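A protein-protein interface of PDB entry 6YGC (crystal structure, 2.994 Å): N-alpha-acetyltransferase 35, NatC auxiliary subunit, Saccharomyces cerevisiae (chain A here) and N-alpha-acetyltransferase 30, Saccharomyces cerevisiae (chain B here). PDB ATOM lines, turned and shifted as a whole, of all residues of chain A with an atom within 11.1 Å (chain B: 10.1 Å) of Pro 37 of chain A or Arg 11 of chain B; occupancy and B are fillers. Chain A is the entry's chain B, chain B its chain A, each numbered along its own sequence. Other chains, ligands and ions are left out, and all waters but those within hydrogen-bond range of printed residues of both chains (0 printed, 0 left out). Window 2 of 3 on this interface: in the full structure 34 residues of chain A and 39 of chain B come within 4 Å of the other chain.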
ATOM      1  N   LEU A  31       4.263 -41.019 -14.460  1.00  0.00           N
ATOM      2  CA  LEU A  31       3.613 -40.675 -13.200  1.00  0.00           C
ATOM      3  C   LEU A  31       3.114 -39.236 -13.208  1.00  0.00           C
ATOM      4  O   LEU A  31       2.004 -38.956 -12.740  1.00  0.00           O
ATOM      5  CB  LEU A  31       4.567 -40.905 -12.029  1.00  0.00           C
ATOM      6  CG  LEU A  31       4.390 -42.224 -11.275  1.00  0.00           C
ATOM      7  CD1 LEU A  31       5.182 -42.192  -9.984  1.00  0.00           C
ATOM      8  CD2 LEU A  31       2.919 -42.494 -10.999  1.00  0.00           C
ATOM      9  N   CYS A  32       3.922 -38.307 -13.724  1.00  0.00           N
ATOM     10  CA  CYS A  32       3.464 -36.927 -13.848  1.00  0.00           C
ATOM     11  C   CYS A  32       2.350 -36.802 -14.877  1.00  0.00           C
ATOM     12  O   CYS A  32       1.457 -35.962 -14.725  1.00  0.00           O
ATOM     13  CB  CYS A  32       4.633 -36.013 -14.213  1.00  0.00           C
ATOM     14  SG  CYS A  32       5.899 -35.894 -12.931  1.00  0.00           S
ATOM     15  N   SER A  33       2.386 -37.626 -15.927  1.00  0.00           N
ATOM     16  CA  SER A  33       1.268 -37.699 -16.859  1.00  0.00           C
ATOM     17  C   SER A  33       0.009 -38.235 -16.192  1.00  0.00           C
ATOM     18  O   SER A  33      -1.099 -37.973 -16.672  1.00  0.00           O
ATOM     19  CB  SER A  33       1.641 -38.575 -18.056  1.00  0.00           C
ATOM     20  OG  SER A  33       0.490 -38.992 -18.770  1.00  0.00           O
ATOM     21  N   LYS A  34       0.159 -38.978 -15.094  1.00  0.00           N
ATOM     22  CA  LYS A  34      -0.989 -39.535 -14.388  1.00  0.00           C
ATOM     23  C   LYS A  34      -1.653 -38.509 -13.476  1.00  0.00           C
ATOM     24  O   LYS A  34      -2.852 -38.619 -13.194  1.00  0.00           O
ATOM     25  CB  LYS A  34      -0.542 -40.762 -13.587  1.00  0.00           C
ATOM     26  CG  LYS A  34      -1.632 -41.476 -12.809  1.00  0.00           C
ATOM     27  CD  LYS A  34      -1.037 -42.615 -11.999  1.00  0.00           C
ATOM     28  CE  LYS A  34      -2.056 -43.226 -11.055  1.00  0.00           C
ATOM     29  NZ  LYS A  34      -1.447 -44.275 -10.191  1.00  0.00           N
ATOM     30  N   LEU A  35      -0.904 -37.506 -13.024  1.00  0.00           N
ATOM     31  CA  LEU A  35      -1.443 -36.515 -12.106  1.00  0.00           C
ATOM     32  C   LEU A  35      -2.429 -35.589 -12.810  1.00  0.00           C
ATOM     33  O   LEU A  35      -2.350 -35.360 -14.020  1.00  0.00           O
ATOM     34  CB  LEU A  35      -0.314 -35.685 -11.492  1.00  0.00           C
ATOM     35  CG  LEU A  35       0.726 -36.412 -10.640  1.00  0.00           C
ATOM     36  CD1 LEU A  35       1.844 -35.457 -10.260  1.00  0.00           C
ATOM     37  CD2 LEU A  35       0.086 -37.013  -9.398  1.00  0.00           C
ATOM     38  N   LYS A  36      -3.367 -35.058 -12.032  1.00  0.00           N
ATOM     39  CA  LYS A  36      -4.264 -34.037 -12.541  1.00  0.00           C
ATOM     40  C   LYS A  36      -3.491 -32.740 -12.778  1.00  0.00           C
ATOM     41  O   LYS A  36      -2.532 -32.441 -12.061  1.00  0.00           O
ATOM     42  CB  LYS A  36      -5.409 -33.791 -11.562  1.00  0.00           C
ATOM     43  CG  LYS A  36      -6.350 -34.974 -11.392  1.00  0.00           C
ATOM     44  CD  LYS A  36      -7.551 -34.602 -10.536  1.00  0.00           C
ATOM     45  CE  LYS A  36      -8.529 -35.760 -10.414  1.00  0.00           C
ATOM     46  NZ  LYS A  36      -9.741 -35.384  -9.634  1.00  0.00           N
ATOM     47  N   PRO A  37      -3.890 -31.949 -13.780  1.00  0.00           N
ATOM     48  CA  PRO A  37      -3.110 -30.746 -14.114  1.00  0.00           C
ATOM     49  C   PRO A  37      -3.003 -29.742 -12.979  1.00  0.00           C
ATOM     50  O   PRO A  37      -1.992 -29.034 -12.888  1.00  0.00           O
ATOM     51  CB  PRO A  37      -3.867 -30.161 -15.316  1.00  0.00           C
ATOM     52  CG  PRO A  37      -5.243 -30.742 -15.226  1.00  0.00           C
ATOM     53  CD  PRO A  37      -5.059 -32.114 -14.660  1.00  0.00           C
ATOM     54  N   GLU A  38      -4.002 -29.664 -12.100  1.00  0.00           N
ATOM     55  CA  GLU A  38      -3.976 -28.672 -11.033  1.00  0.00           C
ATOM     56  C   GLU A  38      -3.111 -29.091  -9.853  1.00  0.00           C
ATOM     57  O   GLU A  38      -2.650 -28.225  -9.101  1.00  0.00           O
ATOM     58  CB  GLU A  38      -5.397 -28.379 -10.548  1.00  0.00           C
ATOM     59  CG  GLU A  38      -6.127 -29.581  -9.962  1.00  0.00           C
ATOM     60  CD  GLU A  38      -7.038 -30.262 -10.965  1.00  0.00           C
ATOM     61  OE1 GLU A  38      -6.783 -30.145 -12.182  1.00  0.00           O
ATOM     62  OE2 GLU A  38      -8.018 -30.907 -10.534  1.00  0.00           O
ATOM     63  N   ALA A  39      -2.875 -30.387  -9.676  1.00  0.00           N
ATOM     64  CA  ALA A  39      -2.213 -30.879  -8.478  1.00  0.00           C
ATOM     65  C   ALA A  39      -0.706 -30.650  -8.532  1.00  0.00           C
ATOM     66  O   ALA A  39      -0.093 -30.636  -9.603  1.00  0.00           O
ATOM     67  CB  ALA A  39      -2.501 -32.367  -8.278  1.00  0.00           C
ATOM     68  N   ILE A  40      -0.115 -30.475  -7.352  1.00  0.00           N
ATOM     69  CA  ILE A  40       1.329 -30.353  -7.185  1.00  0.00           C
ATOM     70  C   ILE A  40       1.751 -31.312  -6.083  1.00  0.00           C
ATOM     71  O   ILE A  40       1.257 -31.219  -4.954  1.00  0.00           O
ATOM     72  CB  ILE A  40       1.757 -28.918  -6.836  1.00  0.00           C
ATOM     73  CG1 ILE A  40       1.359 -27.946  -7.947  1.00  0.00           C
ATOM     74  CG2 ILE A  40       3.258 -28.860  -6.583  1.00  0.00           C
ATOM     75  CD1 ILE A  40       1.753 -26.514  -7.662  1.00  0.00           C
ATOM     76  N   VAL A  41       2.653 -32.232  -6.407  1.00  0.00           N
ATOM     77  CA  VAL A  41       3.177 -33.166  -5.417  1.00  0.00           C
ATOM     78  C   VAL A  41       4.283 -32.479  -4.632  1.00  0.00           C
ATOM     79  O   VAL A  41       5.239 -31.956  -5.214  1.00  0.00           O
ATOM     80  CB  VAL A  41       3.691 -34.446  -6.091  1.00  0.00           C
ATOM     81  CG1 VAL A  41       4.593 -35.216  -5.141  1.00  0.00           C
ATOM     82  CG2 VAL A  41       2.525 -35.311  -6.536  1.00  0.00           C
ATOM     83  N   LEU A  48       4.354 -23.499  -0.425  1.00  0.00           N
ATOM     84  CA  LEU A  48       4.736 -23.189  -1.798  1.00  0.00           C
ATOM     85  C   LEU A  48       5.233 -21.758  -1.962  1.00  0.00           C
ATOM     86  O   LEU A  48       5.847 -21.446  -2.987  1.00  0.00           O
ATOM     87  CB  LEU A  48       3.564 -23.443  -2.745  1.00  0.00           C
ATOM     88  CG  LEU A  48       3.371 -24.898  -3.174  1.00  0.00           C
ATOM     89  CD1 LEU A  48       2.188 -25.032  -4.116  1.00  0.00           C
ATOM     90  CD2 LEU A  48       4.638 -25.430  -3.824  1.00  0.00           C
ATOM     91  N   PRO B   7     -12.551 -16.321 -15.983  1.00  0.00           N
ATOM     92  CA  PRO B   7     -11.768 -16.919 -14.900  1.00  0.00           C
ATOM     93  C   PRO B   7     -10.788 -17.935 -15.461  1.00  0.00           C
ATOM     94  O   PRO B   7     -11.049 -18.588 -16.475  1.00  0.00           O
ATOM     95  CB  PRO B   7     -12.825 -17.593 -14.016  1.00  0.00           C
ATOM     96  CG  PRO B   7     -14.139 -16.999 -14.444  1.00  0.00           C
ATOM     97  CD  PRO B   7     -13.977 -16.671 -15.892  1.00  0.00           C
ATOM     98  N   LEU B   8      -9.646 -18.061 -14.788  1.00  0.00           N
ATOM     99  CA  LEU B   8      -8.595 -18.953 -15.262  1.00  0.00           C
ATOM    100  C   LEU B   8      -9.082 -20.394 -15.316  1.00  0.00           C
ATOM    101  O   LEU B   8      -9.684 -20.898 -14.363  1.00  0.00           O
ATOM    102  CB  LEU B   8      -7.368 -18.855 -14.358  1.00  0.00           C
ATOM    103  CG  LEU B   8      -6.369 -20.007 -14.507  1.00  0.00           C
ATOM    104  CD1 LEU B   8      -5.618 -19.917 -15.829  1.00  0.00           C
ATOM    105  CD2 LEU B   8      -5.409 -20.056 -13.331  1.00  0.00           C
ATOM    106  N   ASP B   9      -8.823 -21.054 -16.441  1.00  0.00           N
ATOM    107  CA  ASP B   9      -9.060 -22.486 -16.579  1.00  0.00           C
ATOM    108  C   ASP B   9      -7.761 -23.205 -16.237  1.00  0.00           C
ATOM    109  O   ASP B   9      -6.806 -23.183 -17.021  1.00  0.00           O
ATOM    110  CB  ASP B   9      -9.533 -22.827 -17.989  1.00  0.00           C
ATOM    111  CG  ASP B   9     -10.056 -24.244 -18.103  1.00  0.00           C
ATOM    112  OD1 ASP B   9     -10.186 -24.918 -17.059  1.00  0.00           O
ATOM    113  OD2 ASP B   9     -10.335 -24.685 -19.237  1.00  0.00           O
ATOM    114  N   ILE B  10      -7.724 -23.833 -15.060  1.00  0.00           N
ATOM    115  CA  ILE B  10      -6.480 -24.420 -14.570  1.00  0.00           C
ATOM    116  C   ILE B  10      -6.034 -25.585 -15.447  1.00  0.00           C
ATOM    117  O   ILE B  10      -4.830 -25.835 -15.589  1.00  0.00           O
ATOM    118  CB  ILE B  10      -6.644 -24.840 -13.097  1.00  0.00           C
ATOM    119  CG1 ILE B  10      -5.329 -25.394 -12.544  1.00  0.00           C
ATOM    120  CG2 ILE B  10      -7.776 -25.851 -12.946  1.00  0.00           C
ATOM    121  CD1 ILE B  10      -4.180 -24.407 -12.596  1.00  0.00           C
ATOM    122  N   ARG B  11      -6.975 -26.308 -16.057  1.00  0.00           N
ATOM    123  CA  ARG B  11      -6.601 -27.446 -16.889  1.00  0.00           C
ATOM    124  C   ARG B  11      -6.053 -27.015 -18.242  1.00  0.00           C
ATOM    125  O   ARG B  11      -5.324 -27.785 -18.878  1.00  0.00           O
ATOM    126  CB  ARG B  11      -7.799 -28.373 -17.078  1.00  0.00           C
ATOM    127  CG  ARG B  11      -8.463 -28.773 -15.778  1.00  0.00           C
ATOM    128  CD  ARG B  11      -9.553 -29.800 -16.000  1.00  0.00           C
ATOM    129  NE  ARG B  11     -10.080 -30.306 -14.737  1.00  0.00           N
ATOM    130  CZ  ARG B  11      -9.513 -31.278 -14.029  1.00  0.00           C
ATOM    131  NH1 ARG B  11      -8.396 -31.848 -14.460  1.00  0.00           N
ATOM    132  NH2 ARG B  11     -10.061 -31.677 -12.890  1.00  0.00           N
ATOM    133  N   ASN B  12      -6.382 -25.807 -18.689  1.00  0.00           N
ATOM    134  CA  ASN B  12      -5.910 -25.293 -19.972  1.00  0.00           C
ATOM    135  C   ASN B  12      -4.470 -24.827 -19.799  1.00  0.00           C
ATOM    136  O   ASN B  12      -4.211 -23.754 -19.249  1.00  0.00           O
ATOM    137  CB  ASN B  12      -6.816 -24.168 -20.459  1.00  0.00           C
ATOM    138  CG  ASN B  12      -6.601 -23.838 -21.920  1.00  0.00           C
ATOM    139  OD1 ASN B  12      -5.471 -23.803 -22.400  1.00  0.00           O
ATOM    140  ND2 ASN B  12      -7.691 -23.597 -22.637  1.00  0.00           N
ATOM    141  N   GLU B  13      -3.522 -25.636 -20.276  1.00  0.00           N
ATOM    142  CA  GLU B  13      -2.111 -25.337 -20.064  1.00  0.00           C
ATOM    143  C   GLU B  13      -1.557 -24.365 -21.100  1.00  0.00           C
ATOM    144  O   GLU B  13      -0.646 -23.592 -20.785  1.00  0.00           O
ATOM    145  CB  GLU B  13      -1.300 -26.633 -20.057  1.00  0.00           C
ATOM    146  CG  GLU B  13      -1.384 -27.393 -18.742  1.00  0.00           C
ATOM    147  CD  GLU B  13      -1.247 -28.891 -18.919  1.00  0.00           C
ATOM    148  OE1 GLU B  13      -1.443 -29.376 -20.052  1.00  0.00           O
ATOM    149  OE2 GLU B  13      -0.945 -29.583 -17.923  1.00  0.00           O
ATOM    150  N   GLU B  14      -2.076 -24.384 -22.331  1.00  0.00           N
ATOM    151  CA  GLU B  14      -1.654 -23.380 -23.304  1.00  0.00           C
ATOM    152  C   GLU B  14      -2.153 -21.994 -22.913  1.00  0.00           C
ATOM    153  O   GLU B  14      -1.523 -20.987 -23.258  1.00  0.00           O
ATOM    154  CB  GLU B  14      -2.135 -23.755 -24.708  1.00  0.00           C
ATOM    155  CG  GLU B  14      -3.638 -23.665 -24.916  1.00  0.00           C
ATOM    156  CD  GLU B  14      -4.042 -23.870 -26.363  1.00  0.00           C
ATOM    157  OE1 GLU B  14      -3.154 -24.147 -27.196  1.00  0.00           O
ATOM    158  OE2 GLU B  14      -5.248 -23.751 -26.668  1.00  0.00           O
ATOM    159  N   GLN B  15      -3.277 -21.924 -22.197  1.00  0.00           N
ATOM    160  CA  GLN B  15      -3.700 -20.664 -21.599  1.00  0.00           C
ATOM    161  C   GLN B  15      -2.796 -20.292 -20.431  1.00  0.00           C
ATOM    162  O   GLN B  15      -2.451 -19.118 -20.251  1.00  0.00           O
ATOM    163  CB  GLN B  15      -5.159 -20.771 -21.149  1.00  0.00           C
ATOM    164  CG  GLN B  15      -5.759 -19.494 -20.590  1.00  0.00           C
ATOM    165  CD  GLN B  15      -7.146 -19.717 -20.016  1.00  0.00           C
ATOM    166  OE1 GLN B  15      -7.303 -19.949 -18.817  1.00  0.00           O
ATOM    167  NE2 GLN B  15      -8.160 -19.650 -20.872  1.00  0.00           N
ATOM    168  N   PHE B  16      -2.397 -21.287 -19.633  1.00  0.00           N
ATOM    169  CA  PHE B  16      -1.438 -21.060 -18.557  1.00  0.00           C
ATOM    170  C   PHE B  16      -0.118 -20.529 -19.101  1.00  0.00           C
ATOM    171  O   PHE B  16       0.462 -19.590 -18.541  1.00  0.00           O
ATOM    172  CB  PHE B  16      -1.224 -22.365 -17.783  1.00  0.00           C
ATOM    173  CG  PHE B  16      -0.166 -22.287 -16.713  1.00  0.00           C
ATOM    174  CD1 PHE B  16       1.169 -22.520 -17.013  1.00  0.00           C
ATOM    175  CD2 PHE B  16      -0.510 -22.018 -15.401  1.00  0.00           C
ATOM    176  CE1 PHE B  16       2.139 -22.456 -16.032  1.00  0.00           C
ATOM    177  CE2 PHE B  16       0.455 -21.956 -14.413  1.00  0.00           C
ATOM    178  CZ  PHE B  16       1.781 -22.176 -14.729  1.00  0.00           C
ATOM    179  N   ALA B  17       0.376 -21.121 -20.192  1.00  0.00           N
ATOM    180  CA  ALA B  17       1.654 -20.696 -20.752  1.00  0.00           C
ATOM    181  C   ALA B  17       1.572 -19.299 -21.350  1.00  0.00           C
ATOM    182  O   ALA B  17       2.550 -18.546 -21.296  1.00  0.00           O
ATOM    183  CB  ALA B  17       2.126 -21.698 -21.806  1.00  0.00           C
ATOM    184  N   ILE B  19      -0.265 -16.930 -20.180  1.00  0.00           N
ATOM    185  CA  ILE B  19      -0.252 -16.008 -19.046  1.00  0.00           C
ATOM    186  C   ILE B  19       1.182 -15.677 -18.657  1.00  0.00           C
ATOM    187  O   ILE B  19       1.553 -14.505 -18.521  1.00  0.00           O
ATOM    188  CB  ILE B  19      -1.034 -16.601 -17.860  1.00  0.00           C
ATOM    189  CG1 ILE B  19      -2.522 -16.699 -18.194  1.00  0.00           C
ATOM    190  CG2 ILE B  19      -0.817 -15.762 -16.608  1.00  0.00           C
ATOM    191  CD1 ILE B  19      -3.352 -17.298 -17.084  1.00  0.00           C
ATOM    192  N   ARG B  37       2.959 -21.149 -10.262  1.00  0.00           N
ATOM    193  CA  ARG B  37       2.220 -22.257  -9.671  1.00  0.00           C
ATOM    194  C   ARG B  37       1.918 -22.033  -8.195  1.00  0.00           C
ATOM    195  O   ARG B  37       1.048 -22.715  -7.645  1.00  0.00           O
ATOM    196  CB  ARG B  37       2.982 -23.570  -9.860  1.00  0.00           C
ATOM    197  CG  ARG B  37       2.965 -24.089 -11.292  1.00  0.00           C
ATOM    198  CD  ARG B  37       2.679 -25.583 -11.336  1.00  0.00           C
ATOM    199  NE  ARG B  37       2.585 -26.089 -12.703  1.00  0.00           N
ATOM    200  CZ  ARG B  37       1.470 -26.088 -13.428  1.00  0.00           C
ATOM    201  NH1 ARG B  37       0.347 -25.603 -12.919  1.00  0.00           N
ATOM    202  NH2 ARG B  37       1.479 -26.569 -14.663  1.00  0.00           N
ATOM    203  N   LEU B  40      -1.409 -19.599  -9.079  1.00  0.00           N
ATOM    204  CA  LEU B  40      -2.493 -20.141  -9.889  1.00  0.00           C
ATOM    205  C   LEU B  40      -2.984 -21.492  -9.376  1.00  0.00           C
ATOM    206  O   LEU B  40      -4.190 -21.760  -9.401  1.00  0.00           O
ATOM    207  CB  LEU B  40      -2.045 -20.254 -11.350  1.00  0.00           C
ATOM    208  CG  LEU B  40      -2.092 -18.978 -12.205  1.00  0.00           C
ATOM    209  CD1 LEU B  40      -1.093 -17.921 -11.748  1.00  0.00           C
ATOM    210  CD2 LEU B  40      -1.881 -19.303 -13.677  1.00  0.00           C
ATOM    211  N   ASN B  41      -2.081 -22.354  -8.904  1.00  0.00           N
ATOM    212  CA  ASN B  41      -2.510 -23.683  -8.476  1.00  0.00           C
ATOM    213  C   ASN B  41      -3.226 -23.631  -7.130  1.00  0.00           C
ATOM    214  O   ASN B  41      -4.189 -24.373  -6.905  1.00  0.00           O
ATOM    215  CB  ASN B  41      -1.314 -24.630  -8.415  1.00  0.00           C
ATOM    216  CG  ASN B  41      -0.873 -25.100  -9.789  1.00  0.00           C
ATOM    217  OD1 ASN B  41      -0.257 -24.349 -10.545  1.00  0.00           O
ATOM    218  ND2 ASN B  41      -1.179 -26.352 -10.115  1.00  0.00           N
ATOM    219  N   GLN B  42      -2.777 -22.761  -6.227  1.00  0.00           N
ATOM    220  CA  GLN B  42      -3.387 -22.633  -4.910  1.00  0.00           C
ATOM    221  C   GLN B  42      -4.593 -21.705  -4.901  1.00  0.00           C
ATOM    222  O   GLN B  42      -5.547 -21.953  -4.152  1.00  0.00           O
ATOM    223  CB  GLN B  42      -2.350 -22.139  -3.895  1.00  0.00           C
ATOM    224  CG  GLN B  42      -1.298 -23.178  -3.557  1.00  0.00           C
ATOM    225  CD  GLN B  42      -0.261 -22.665  -2.577  1.00  0.00           C
ATOM    226  OE1 GLN B  42       0.244 -23.414  -1.743  1.00  0.00           O
ATOM    227  NE2 GLN B  42       0.065 -21.383  -2.680  1.00  0.00           N
ATOM    228  N   PRO B  44      -6.757 -20.737  -7.836  1.00  0.00           N
ATOM    229  CA  PRO B  44      -7.188 -20.699  -9.241  1.00  0.00           C
ATOM    230  C   PRO B  44      -8.320 -19.722  -9.493  1.00  0.00           C
ATOM    231  O   PRO B  44      -8.387 -19.135 -10.580  1.00  0.00           O
ATOM    232  CB  PRO B  44      -7.624 -22.147  -9.521  1.00  0.00           C
ATOM    233  CG  PRO B  44      -7.062 -22.960  -8.390  1.00  0.00           C
ATOM    234  CD  PRO B  44      -7.039 -22.041  -7.215  1.00  0.00           C
ATOM    235  N   ASN B  59      -9.139 -16.949 -28.144  1.00  0.00           N
ATOM    236  CA  ASN B  59      -8.922 -17.383 -26.771  1.00  0.00           C
ATOM    237  C   ASN B  59      -7.566 -16.975 -26.205  1.00  0.00           C
ATOM    238  O   ASN B  59      -7.328 -17.185 -25.011  1.00  0.00           O
ATOM    239  CB  ASN B  59      -9.082 -18.905 -26.666  1.00  0.00           C
ATOM    240  CG  ASN B  59      -9.251 -19.379 -25.231  1.00  0.00           C
ATOM    241  OD1 ASN B  59      -8.295 -19.820 -24.593  1.00  0.00           O
ATOM    242  ND2 ASN B  59     -10.471 -19.275 -24.714  1.00  0.00           N
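The guanidinium group (NH2) of Arg 11 of chain B lies within salt-bridge range of the side-chain carboxylate (OE2) of Glu 38 of chain A (3.2 Å).
ND2 of Asn 41 of chain B is in hydrogen-bond range of O of Glu 38 of chain A (2.6 Å).
The guanidinium group (NH1) of Arg 37 of chain B lies within hydrogen-bond range of the side-chain amide oxygen (OD1) of Asn 41 of chain B, at 2.8 Å.
Among the printed residues, merely in contact across the chains: Pro 37 of chain A with Arg 11 of chain B, Pro 37 of chain A with Glu 13 of chain B, Pro 37 of chain A with Asn 41 of chain B, Glu 38 of chain A with Ile 10 of chain B, Ile 40 of chain A with Arg 37 of chain B, Ile 40 of chain A with Asn 41 of chain B and Leu 48 of chain A with Gln 42 of chain B.
Pro 37 of chain A touches three residues of chain B.
No residue of chain B comes within 4 Å of Lys 36 of chain A.
Of chain B, only Ile 10 (3.6 Å), Arg 11 (3.2 Å) and Asn 41 (2.6 Å) come within 4 Å of Glu 38 of chain A.
Asp 9 of chain B touches none of the printed residues of chain A.
Of the printed residues of chain A, Glu 13 of chain B touches Pro 37.
Of the printed residues of chain B, Leu 48 of chain A touches Gln 42 (3.5 Å).
Of the printed residues of chain A, Asn 41 of chain B touches Pro 37 (3.9 Å), Glu 38 (2.6 Å) and Ile 40 (3.7 Å).
Leu 8 of chain B touches none of the printed residues of chain A.
The nearest residue of chain B that does not touch Pro 37 of chain A is Arg 37 of chain B (4.2 Å).
The nearest residue of chain A that does not touch Arg 11 of chain B is Lys 36 of chain A (4.5 Å).
Hydrophobic or aromatic side chains of chain B within 4 Å of the printed part of chain A: Ile 10.
Along chain B the printed residues that touch a printed residue of chain A span positions 10 to 42.
Printed residues of chain A that touch a printed residue of chain B: Pro 37, Glu 38, Ile 40 and Leu 48.
Hydrophobic or aromatic side chains of chain A that line the printed part of chain B: Pro 37, Ile 40 and Leu 48.
Among the printed residues, Asp or Glu carboxylates within 4 Å of a Lys or Arg side-chain nitrogen of the other chain: Glu 38 of chain A with Arg 11 of chain B (3.2 Å).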
